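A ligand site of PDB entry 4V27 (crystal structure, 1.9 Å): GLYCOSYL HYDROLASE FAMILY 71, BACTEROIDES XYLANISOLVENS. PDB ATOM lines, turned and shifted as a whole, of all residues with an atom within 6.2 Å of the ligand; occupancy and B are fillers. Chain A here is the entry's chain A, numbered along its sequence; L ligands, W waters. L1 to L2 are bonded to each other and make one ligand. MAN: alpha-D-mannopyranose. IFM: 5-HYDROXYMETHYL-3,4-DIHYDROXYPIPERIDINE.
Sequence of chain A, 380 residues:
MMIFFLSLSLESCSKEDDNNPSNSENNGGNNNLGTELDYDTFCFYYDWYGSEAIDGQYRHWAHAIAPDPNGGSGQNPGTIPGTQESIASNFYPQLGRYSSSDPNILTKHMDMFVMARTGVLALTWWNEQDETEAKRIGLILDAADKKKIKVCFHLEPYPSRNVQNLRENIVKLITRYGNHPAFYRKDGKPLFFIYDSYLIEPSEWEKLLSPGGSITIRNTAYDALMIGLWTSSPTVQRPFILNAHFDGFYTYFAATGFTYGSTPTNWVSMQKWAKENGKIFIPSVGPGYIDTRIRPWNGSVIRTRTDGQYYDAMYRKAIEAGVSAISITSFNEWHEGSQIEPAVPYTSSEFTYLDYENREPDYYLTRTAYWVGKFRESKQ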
ATOM      1  N   PHE A  44     -29.116 -32.212  -4.856  1.00  0.00           N
ATOM      2  CA  PHE A  44     -27.708 -32.251  -4.421  1.00  0.00           C
ATOM      3  C   PHE A  44     -27.468 -31.367  -3.193  1.00  0.00           C
ATOM      4  O   PHE A  44     -27.720 -30.156  -3.208  1.00  0.00           O
ATOM      5  CB  PHE A  44     -26.730 -31.915  -5.560  1.00  0.00           C
ATOM      6  CG  PHE A  44     -26.704 -32.952  -6.646  1.00  0.00           C
ATOM      7  CD1 PHE A  44     -26.202 -34.232  -6.387  1.00  0.00           C
ATOM      8  CD2 PHE A  44     -27.185 -32.669  -7.911  1.00  0.00           C
ATOM      9  CE1 PHE A  44     -26.191 -35.209  -7.372  1.00  0.00           C
ATOM     10  CE2 PHE A  44     -27.182 -33.642  -8.919  1.00  0.00           C
ATOM     11  CZ  PHE A  44     -26.677 -34.905  -8.644  1.00  0.00           C
ATOM     12  N   TYR A  46     -25.056 -30.315   0.289  1.00  0.00           N
ATOM     13  CA  TYR A  46     -23.691 -30.083   0.779  1.00  0.00           C
ATOM     14  C   TYR A  46     -23.689 -29.906   2.292  1.00  0.00           C
ATOM     15  O   TYR A  46     -24.431 -29.076   2.829  1.00  0.00           O
ATOM     16  CB  TYR A  46     -23.062 -28.899   0.020  1.00  0.00           C
ATOM     17  CG  TYR A  46     -22.992 -29.277  -1.437  1.00  0.00           C
ATOM     18  CD1 TYR A  46     -24.103 -29.093  -2.281  1.00  0.00           C
ATOM     19  CD2 TYR A  46     -21.871 -29.923  -1.958  1.00  0.00           C
ATOM     20  CE1 TYR A  46     -24.066 -29.506  -3.609  1.00  0.00           C
ATOM     21  CE2 TYR A  46     -21.834 -30.337  -3.286  1.00  0.00           C
ATOM     22  CZ  TYR A  46     -22.927 -30.124  -4.104  1.00  0.00           C
ATOM     23  OH  TYR A  46     -22.897 -30.542  -5.426  1.00  0.00           O
ATOM     24  N   TRP A  48     -20.863 -29.210   4.194  1.00  0.00           N
ATOM     25  CA  TRP A  48     -19.528 -28.736   4.480  1.00  0.00           C
ATOM     26  C   TRP A  48     -19.461 -27.367   5.139  1.00  0.00           C
ATOM     27  O   TRP A  48     -18.390 -26.767   5.246  1.00  0.00           O
ATOM     28  CB  TRP A  48     -18.676 -28.822   3.222  1.00  0.00           C
ATOM     29  CG  TRP A  48     -19.203 -28.048   2.022  1.00  0.00           C
ATOM     30  CD1 TRP A  48     -20.033 -26.928   2.012  1.00  0.00           C
ATOM     31  CD2 TRP A  48     -18.888 -28.310   0.606  1.00  0.00           C
ATOM     32  NE1 TRP A  48     -20.267 -26.509   0.718  1.00  0.00           N
ATOM     33  CE2 TRP A  48     -19.612 -27.277  -0.167  1.00  0.00           C
ATOM     34  CE3 TRP A  48     -18.118 -29.245  -0.067  1.00  0.00           C
ATOM     35  CZ2 TRP A  48     -19.536 -27.213  -1.550  1.00  0.00           C
ATOM     36  CZ3 TRP A  48     -18.056 -29.180  -1.468  1.00  0.00           C
ATOM     37  CH2 TRP A  48     -18.735 -28.185  -2.197  1.00  0.00           C
ATOM     38  N   HIS A  60     -16.349 -23.210   5.004  1.00  0.00           N
ATOM     39  CA  HIS A  60     -16.982 -22.916   3.701  1.00  0.00           C
ATOM     40  C   HIS A  60     -17.589 -21.541   3.548  1.00  0.00           C
ATOM     41  O   HIS A  60     -17.480 -20.967   2.470  1.00  0.00           O
ATOM     42  CB  HIS A  60     -17.904 -24.052   3.208  1.00  0.00           C
ATOM     43  CG  HIS A  60     -17.156 -25.156   2.479  1.00  0.00           C
ATOM     44  ND1 HIS A  60     -17.177 -25.292   1.138  1.00  0.00           N
ATOM     45  CD2 HIS A  60     -16.289 -26.153   2.958  1.00  0.00           C
ATOM     46  CE1 HIS A  60     -16.369 -26.330   0.771  1.00  0.00           C
ATOM     47  NE2 HIS A  60     -15.845 -26.855   1.896  1.00  0.00           N
ATOM     48  N   HIS A  63     -13.733 -19.042   2.468  1.00  0.00           N
ATOM     49  CA  HIS A  63     -13.288 -19.803   1.287  1.00  0.00           C
ATOM     50  C   HIS A  63     -12.237 -19.046   0.523  1.00  0.00           C
ATOM     51  O   HIS A  63     -12.306 -17.815   0.395  1.00  0.00           O
ATOM     52  CB  HIS A  63     -14.496 -20.063   0.380  1.00  0.00           C
ATOM     53  CG  HIS A  63     -14.368 -21.257  -0.541  1.00  0.00           C
ATOM     54  ND1 HIS A  63     -13.660 -21.215  -1.700  1.00  0.00           N
ATOM     55  CD2 HIS A  63     -14.941 -22.532  -0.469  1.00  0.00           C
ATOM     56  CE1 HIS A  63     -13.756 -22.414  -2.313  1.00  0.00           C
ATOM     57  NE2 HIS A  63     -14.546 -23.209  -1.554  1.00  0.00           N
ATOM     58  N   THR A 124     -23.043 -34.939  -0.811  1.00  0.00           N
ATOM     59  CA  THR A 124     -21.630 -34.797  -1.197  1.00  0.00           C
ATOM     60  C   THR A 124     -20.794 -35.673  -0.262  1.00  0.00           C
ATOM     61  O   THR A 124     -21.043 -35.679   0.965  1.00  0.00           O
ATOM     62  CB  THR A 124     -21.173 -33.319  -1.110  1.00  0.00           C
ATOM     63  OG1 THR A 124     -19.914 -33.155  -1.780  1.00  0.00           O
ATOM     64  CG2 THR A 124     -21.037 -32.819   0.346  1.00  0.00           C
ATOM     65  N   TRP A 126     -16.698 -36.965   0.412  1.00  0.00           N
ATOM     66  CA  TRP A 126     -15.316 -36.619   0.080  1.00  0.00           C
ATOM     67  C   TRP A 126     -14.255 -37.519   0.647  1.00  0.00           C
ATOM     68  O   TRP A 126     -13.066 -37.201   0.534  1.00  0.00           O
ATOM     69  CB  TRP A 126     -15.035 -35.183   0.504  1.00  0.00           C
ATOM     70  CG  TRP A 126     -15.686 -34.171  -0.392  1.00  0.00           C
ATOM     71  CD1 TRP A 126     -16.947 -33.588  -0.243  1.00  0.00           C
ATOM     72  CD2 TRP A 126     -15.142 -33.587  -1.632  1.00  0.00           C
ATOM     73  NE1 TRP A 126     -17.194 -32.695  -1.263  1.00  0.00           N
ATOM     74  CE2 TRP A 126     -16.152 -32.657  -2.129  1.00  0.00           C
ATOM     75  CE3 TRP A 126     -13.947 -33.745  -2.352  1.00  0.00           C
ATOM     76  CZ2 TRP A 126     -15.981 -31.926  -3.309  1.00  0.00           C
ATOM     77  CZ3 TRP A 126     -13.778 -33.003  -3.525  1.00  0.00           C
ATOM     78  CH2 TRP A 126     -14.769 -32.118  -3.999  1.00  0.00           C
ATOM     79  N   HIS A 154     -23.158 -38.820  -3.235  1.00  0.00           N
ATOM     80  CA  HIS A 154     -22.585 -38.185  -4.416  1.00  0.00           C
ATOM     81  C   HIS A 154     -21.095 -38.265  -4.232  1.00  0.00           C
ATOM     82  O   HIS A 154     -20.515 -37.493  -3.474  1.00  0.00           O
ATOM     83  CB  HIS A 154     -23.051 -36.736  -4.457  1.00  0.00           C
ATOM     84  CG  HIS A 154     -22.745 -36.019  -5.747  1.00  0.00           C
ATOM     85  ND1 HIS A 154     -22.885 -34.678  -5.877  1.00  0.00           N
ATOM     86  CD2 HIS A 154     -22.276 -36.483  -6.966  1.00  0.00           C
ATOM     87  CE1 HIS A 154     -22.554 -34.322  -7.136  1.00  0.00           C
ATOM     88  NE2 HIS A 154     -22.179 -35.427  -7.798  1.00  0.00           N
ATOM     89  N   GLU A 156     -17.439 -37.801  -4.671  1.00  0.00           N
ATOM     90  CA  GLU A 156     -16.700 -36.665  -5.221  1.00  0.00           C
ATOM     91  C   GLU A 156     -15.273 -37.080  -5.603  1.00  0.00           C
ATOM     92  O   GLU A 156     -14.824 -38.150  -5.207  1.00  0.00           O
ATOM     93  CB  GLU A 156     -16.653 -35.543  -4.174  1.00  0.00           C
ATOM     94  CG  GLU A 156     -18.015 -34.994  -3.766  1.00  0.00           C
ATOM     95  CD  GLU A 156     -18.543 -33.940  -4.743  1.00  0.00           C
ATOM     96  OE1 GLU A 156     -17.914 -33.735  -5.817  1.00  0.00           O
ATOM     97  OE2 GLU A 156     -19.582 -33.329  -4.416  1.00  0.00           O
ATOM     98  N   PRO A 157     -14.564 -36.218  -6.339  1.00  0.00           N
ATOM     99  CA  PRO A 157     -13.199 -36.571  -6.766  1.00  0.00           C
ATOM    100  C   PRO A 157     -12.187 -36.390  -5.628  1.00  0.00           C
ATOM    101  O   PRO A 157     -11.422 -35.427  -5.618  1.00  0.00           O
ATOM    102  CB  PRO A 157     -12.907 -35.590  -7.916  1.00  0.00           C
ATOM    103  CG  PRO A 157     -14.138 -34.759  -8.088  1.00  0.00           C
ATOM    104  CD  PRO A 157     -14.965 -34.905  -6.858  1.00  0.00           C
ATOM    105  N   TYR A 195     -19.265 -37.936  -9.432  1.00  0.00           N
ATOM    106  CA  TYR A 195     -18.866 -36.662  -9.996  1.00  0.00           C
ATOM    107  C   TYR A 195     -17.503 -36.797 -10.702  1.00  0.00           C
ATOM    108  O   TYR A 195     -16.631 -37.548 -10.253  1.00  0.00           O
ATOM    109  CB  TYR A 195     -18.857 -35.553  -8.935  1.00  0.00           C
ATOM    110  CG  TYR A 195     -18.633 -34.201  -9.568  1.00  0.00           C
ATOM    111  CD1 TYR A 195     -19.613 -33.636 -10.374  1.00  0.00           C
ATOM    112  CD2 TYR A 195     -17.426 -33.524  -9.407  1.00  0.00           C
ATOM    113  CE1 TYR A 195     -19.411 -32.411 -11.010  1.00  0.00           C
ATOM    114  CE2 TYR A 195     -17.210 -32.299 -10.026  1.00  0.00           C
ATOM    115  CZ  TYR A 195     -18.195 -31.750 -10.833  1.00  0.00           C
ATOM    116  OH  TYR A 195     -17.990 -30.534 -11.455  1.00  0.00           O
ATOM    117  N   ASP A 196     -17.367 -36.099 -11.826  1.00  0.00           N
ATOM    118  CA  ASP A 196     -16.156 -36.145 -12.654  1.00  0.00           C
ATOM    119  C   ASP A 196     -15.661 -37.580 -12.924  1.00  0.00           C
ATOM    120  O   ASP A 196     -14.462 -37.864 -12.840  1.00  0.00           O
ATOM    121  CB  ASP A 196     -15.038 -35.264 -12.046  1.00  0.00           C
ATOM    122  CG  ASP A 196     -15.304 -33.775 -12.253  1.00  0.00           C
ATOM    123  OD1 ASP A 196     -16.284 -33.420 -12.939  1.00  0.00           O
ATOM    124  OD2 ASP A 196     -14.541 -32.946 -11.721  1.00  0.00           O
ATOM    125  N   TYR A 250     -25.859 -38.574 -15.354  1.00  0.00           N
ATOM    126  CA  TYR A 250     -26.450 -37.296 -14.989  1.00  0.00           C
ATOM    127  C   TYR A 250     -25.549 -36.206 -15.551  1.00  0.00           C
ATOM    128  O   TYR A 250     -24.488 -36.513 -16.076  1.00  0.00           O
ATOM    129  CB  TYR A 250     -26.608 -37.171 -13.468  1.00  0.00           C
ATOM    130  CG  TYR A 250     -25.342 -36.952 -12.645  1.00  0.00           C
ATOM    131  CD1 TYR A 250     -24.294 -37.871 -12.666  1.00  0.00           C
ATOM    132  CD2 TYR A 250     -25.232 -35.843 -11.816  1.00  0.00           C
ATOM    133  CE1 TYR A 250     -23.144 -37.676 -11.882  1.00  0.00           C
ATOM    134  CE2 TYR A 250     -24.106 -35.653 -11.030  1.00  0.00           C
ATOM    135  CZ  TYR A 250     -23.072 -36.571 -11.069  1.00  0.00           C
ATOM    136  OH  TYR A 250     -21.962 -36.320 -10.291  1.00  0.00           O
ATOM    137  N   TYR A 252     -25.214 -32.806 -13.972  1.00  0.00           N
ATOM    138  CA  TYR A 252     -24.845 -31.869 -12.881  1.00  0.00           C
ATOM    139  C   TYR A 252     -25.011 -30.349 -13.116  1.00  0.00           C
ATOM    140  O   TYR A 252     -25.715 -29.666 -12.362  1.00  0.00           O
ATOM    141  CB  TYR A 252     -23.461 -32.151 -12.238  1.00  0.00           C
ATOM    142  CG  TYR A 252     -23.327 -31.315 -10.983  1.00  0.00           C
ATOM    143  CD1 TYR A 252     -23.942 -31.721  -9.801  1.00  0.00           C
ATOM    144  CD2 TYR A 252     -22.699 -30.058 -11.002  1.00  0.00           C
ATOM    145  CE1 TYR A 252     -23.897 -30.947  -8.655  1.00  0.00           C
ATOM    146  CE2 TYR A 252     -22.677 -29.251  -9.859  1.00  0.00           C
ATOM    147  CZ  TYR A 252     -23.279 -29.710  -8.683  1.00  0.00           C
ATOM    148  OH  TYR A 252     -23.268 -28.958  -7.509  1.00  0.00           O
ATOM    149  N   ILE A 294     -16.182 -16.450  -5.327  1.00  0.00           N
ATOM    150  CA  ILE A 294     -15.022 -17.340  -5.238  1.00  0.00           C
ATOM    151  C   ILE A 294     -14.229 -17.509  -6.549  1.00  0.00           C
ATOM    152  O   ILE A 294     -13.067 -17.922  -6.508  1.00  0.00           O
ATOM    153  CB  ILE A 294     -15.374 -18.722  -4.611  1.00  0.00           C
ATOM    154  CG1 ILE A 294     -16.418 -19.498  -5.437  1.00  0.00           C
ATOM    155  CG2 ILE A 294     -15.868 -18.537  -3.180  1.00  0.00           C
ATOM    156  CD1 ILE A 294     -16.192 -20.998  -5.434  1.00  0.00           C
ATOM    157  N   ARG A 295     -14.860 -17.210  -7.685  1.00  0.00           N
ATOM    158  CA  ARG A 295     -14.224 -17.308  -9.011  1.00  0.00           C
ATOM    159  C   ARG A 295     -14.520 -16.034  -9.806  1.00  0.00           C
ATOM    160  O   ARG A 295     -15.366 -16.025 -10.726  1.00  0.00           O
ATOM    161  CB  ARG A 295     -14.704 -18.561  -9.757  1.00  0.00           C
ATOM    162  CG  ARG A 295     -14.602 -19.859  -8.938  1.00  0.00           C
ATOM    163  CD  ARG A 295     -14.951 -21.099  -9.743  1.00  0.00           C
ATOM    164  NE  ARG A 295     -14.832 -22.326  -8.954  1.00  0.00           N
ATOM    165  CZ  ARG A 295     -15.849 -23.129  -8.633  1.00  0.00           C
ATOM    166  NH1 ARG A 295     -17.089 -22.856  -9.030  1.00  0.00           N
ATOM    167  NH2 ARG A 295     -15.625 -24.241  -7.924  1.00  0.00           N
ATOM    168  N   GLU A 333     -25.497 -25.525  -2.738  1.00  0.00           N
ATOM    169  CA  GLU A 333     -24.161 -25.152  -3.216  1.00  0.00           C
ATOM    170  C   GLU A 333     -24.127 -23.626  -3.337  1.00  0.00           C
ATOM    171  O   GLU A 333     -24.287 -23.047  -4.427  1.00  0.00           O
ATOM    172  CB  GLU A 333     -23.804 -25.843  -4.541  1.00  0.00           C
ATOM    173  CG  GLU A 333     -22.374 -26.419  -4.597  1.00  0.00           C
ATOM    174  CD  GLU A 333     -21.243 -25.391  -4.449  1.00  0.00           C
ATOM    175  OE1 GLU A 333     -21.498 -24.212  -4.134  1.00  0.00           O
ATOM    176  OE2 GLU A 333     -20.065 -25.771  -4.685  1.00  0.00           O
ATOM    177  N   HIS A 335     -21.761 -21.486  -2.951  1.00  0.00           N
ATOM    178  CA  HIS A 335     -20.622 -20.908  -3.676  1.00  0.00           C
ATOM    179  C   HIS A 335     -20.927 -20.716  -5.133  1.00  0.00           C
ATOM    180  O   HIS A 335     -20.358 -19.845  -5.768  1.00  0.00           O
ATOM    181  CB  HIS A 335     -19.382 -21.786  -3.548  1.00  0.00           C
ATOM    182  CG  HIS A 335     -19.069 -22.185  -2.121  1.00  0.00           C
ATOM    183  ND1 HIS A 335     -18.849 -23.470  -1.754  1.00  0.00           N
ATOM    184  CD2 HIS A 335     -18.961 -21.427  -0.963  1.00  0.00           C
ATOM    185  CE1 HIS A 335     -18.591 -23.525  -0.445  1.00  0.00           C
ATOM    186  NE2 HIS A 335     -18.673 -22.278   0.054  1.00  0.00           N
ATOM    187  N   GLU A 336     -21.831 -21.535  -5.672  1.00  0.00           N
ATOM    188  CA  GLU A 336     -22.092 -21.519  -7.107  1.00  0.00           C
ATOM    189  C   GLU A 336     -23.447 -20.931  -7.468  1.00  0.00           C
ATOM    190  O   GLU A 336     -23.815 -20.879  -8.649  1.00  0.00           O
ATOM    191  CB  GLU A 336     -21.900 -22.942  -7.678  1.00  0.00           C
ATOM    192  CG  GLU A 336     -20.405 -23.282  -7.680  1.00  0.00           C
ATOM    193  CD  GLU A 336     -20.070 -24.732  -7.948  1.00  0.00           C
ATOM    194  OE1 GLU A 336     -20.973 -25.602  -8.004  1.00  0.00           O
ATOM    195  OE2 GLU A 336     -18.870 -25.005  -8.123  1.00  0.00           O
HETATM  196  C1  MAN L   1     -15.439 -27.838  -5.688  1.00  0.00           C
HETATM  197  C2  MAN L   1     -14.302 -28.163  -4.708  1.00  0.00           C
HETATM  198  C3  MAN L   1     -14.634 -27.656  -3.299  1.00  0.00           C
HETATM  199  C4  MAN L   1     -15.095 -26.189  -3.339  1.00  0.00           C
HETATM  200  C5  MAN L   1     -16.231 -26.027  -4.341  1.00  0.00           C
HETATM  201  C6  MAN L   1     -16.680 -24.567  -4.407  1.00  0.00           C
HETATM  202  O2  MAN L   1     -13.182 -27.462  -5.179  1.00  0.00           O
HETATM  203  O3  MAN L   1     -13.510 -27.807  -2.465  1.00  0.00           O
HETATM  204  O4  MAN L   1     -15.504 -25.726  -2.064  1.00  0.00           O
HETATM  205  O5  MAN L   1     -15.781 -26.461  -5.613  1.00  0.00           O
HETATM  206  O6  MAN L   1     -17.818 -24.449  -5.231  1.00  0.00           O
HETATM  207  O4  IFM L   2     -17.207 -31.318  -6.500  1.00  0.00           O
HETATM  208  C4  IFM L   2     -18.161 -30.235  -6.371  1.00  0.00           C
HETATM  209  C3  IFM L   2     -17.406 -28.913  -6.519  1.00  0.00           C
HETATM  210  O3  IFM L   2     -16.476 -28.784  -5.437  1.00  0.00           O
HETATM  211  C2  IFM L   2     -18.354 -27.705  -6.534  1.00  0.00           C
HETATM  212  N   IFM L   2     -19.352 -27.914  -7.569  1.00  0.00           N
HETATM  213  C1  IFM L   2     -20.159 -29.114  -7.426  1.00  0.00           C
HETATM  214  C5  IFM L   2     -19.253 -30.355  -7.436  1.00  0.00           C
HETATM  215  C6  IFM L   2     -20.095 -31.616  -7.296  1.00  0.00           C
HETATM  216  O6  IFM L   2     -20.692 -31.689  -5.985  1.00  0.00           O
HETATM  217  O   HOH W   1     -13.127 -25.403  -6.774  1.00  0.00           O
HETATM  218  O   HOH W   2     -11.191 -26.173  -2.742  1.00  0.00           O
HETATM  219  O   HOH W   3     -18.781 -28.223 -10.300  1.00  0.00           O
HETATM  220  O   HOH W   4     -14.623 -30.957  -7.477  1.00  0.00           O
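The side-chain hydroxyl (OH) of Tyr 46 sits at hydrogen-bond distance from an oxygen (O6) of IFM L2. NH2 of Arg 295 sits at hydrogen-bond distance from O5 of MAN L1 (3.2 Å). The side-chain carboxylate (OE1) of Glu 336 is in salt-bridge range of a nitrogen (N) of IFM L2 (2.9 Å). OE2 of Glu 333 lies within salt-bridge range of N of IFM L2 (3.7 Å). The side-chain carboxylate of Glu 156 sits at hydrogen-bond distance from an oxygen (O6) of IFM L2, at 2.5 Å. NE2 of His 63 sits at hydrogen-bond distance from O4 of MAN L1, 2.7 Å away.
O of His 60 sits at hydrogen-bond distance from NE2 of His 335 (3.0 Å). ND1 of His 60 lies within hydrogen-bond range of NE1 of Trp 48 (3.3 Å). The side-chain hydroxyl (OG1) of Thr 124 is in hydrogen-bond range of the indole nitrogen (NE1) of Trp 126, 2.8 Å away. The side-chain hydroxyl of Tyr 252 sits at hydrogen-bond distance from the side-chain hydroxyl of Tyr 46, 2.6 Å away. A ring nitrogen (NE2) of His 154 is in hydrogen-bond range of the side-chain hydroxyl (OH) of Tyr 250 (2.7 Å). The guanidinium group (NH1) of Arg 295 lies within salt-bridge range of the side-chain carboxylate (OE2) of Glu 336. N of His 335 is in hydrogen-bond range of OE1 of Glu 333, 3.0 Å away. OH of Tyr 250 lies close to N of Tyr 195 (3.3 Å).
Merely in contact with the ligand: His 60, Tyr 252, His 154, Trp 126, His 335, Tyr 195, Ile 294 and Trp 48. Of the 19 residues printed, 14 come within 4 Å of the ligand.
Water W1 bridges an oxygen (O2) of MAN L1 (2.6 Å) and the guanidinium group of Arg 295 (3.0 Å). Water W3 bridges the side-chain hydroxyl (OH) of Tyr 195 and a nitrogen (N) of IFM L2.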
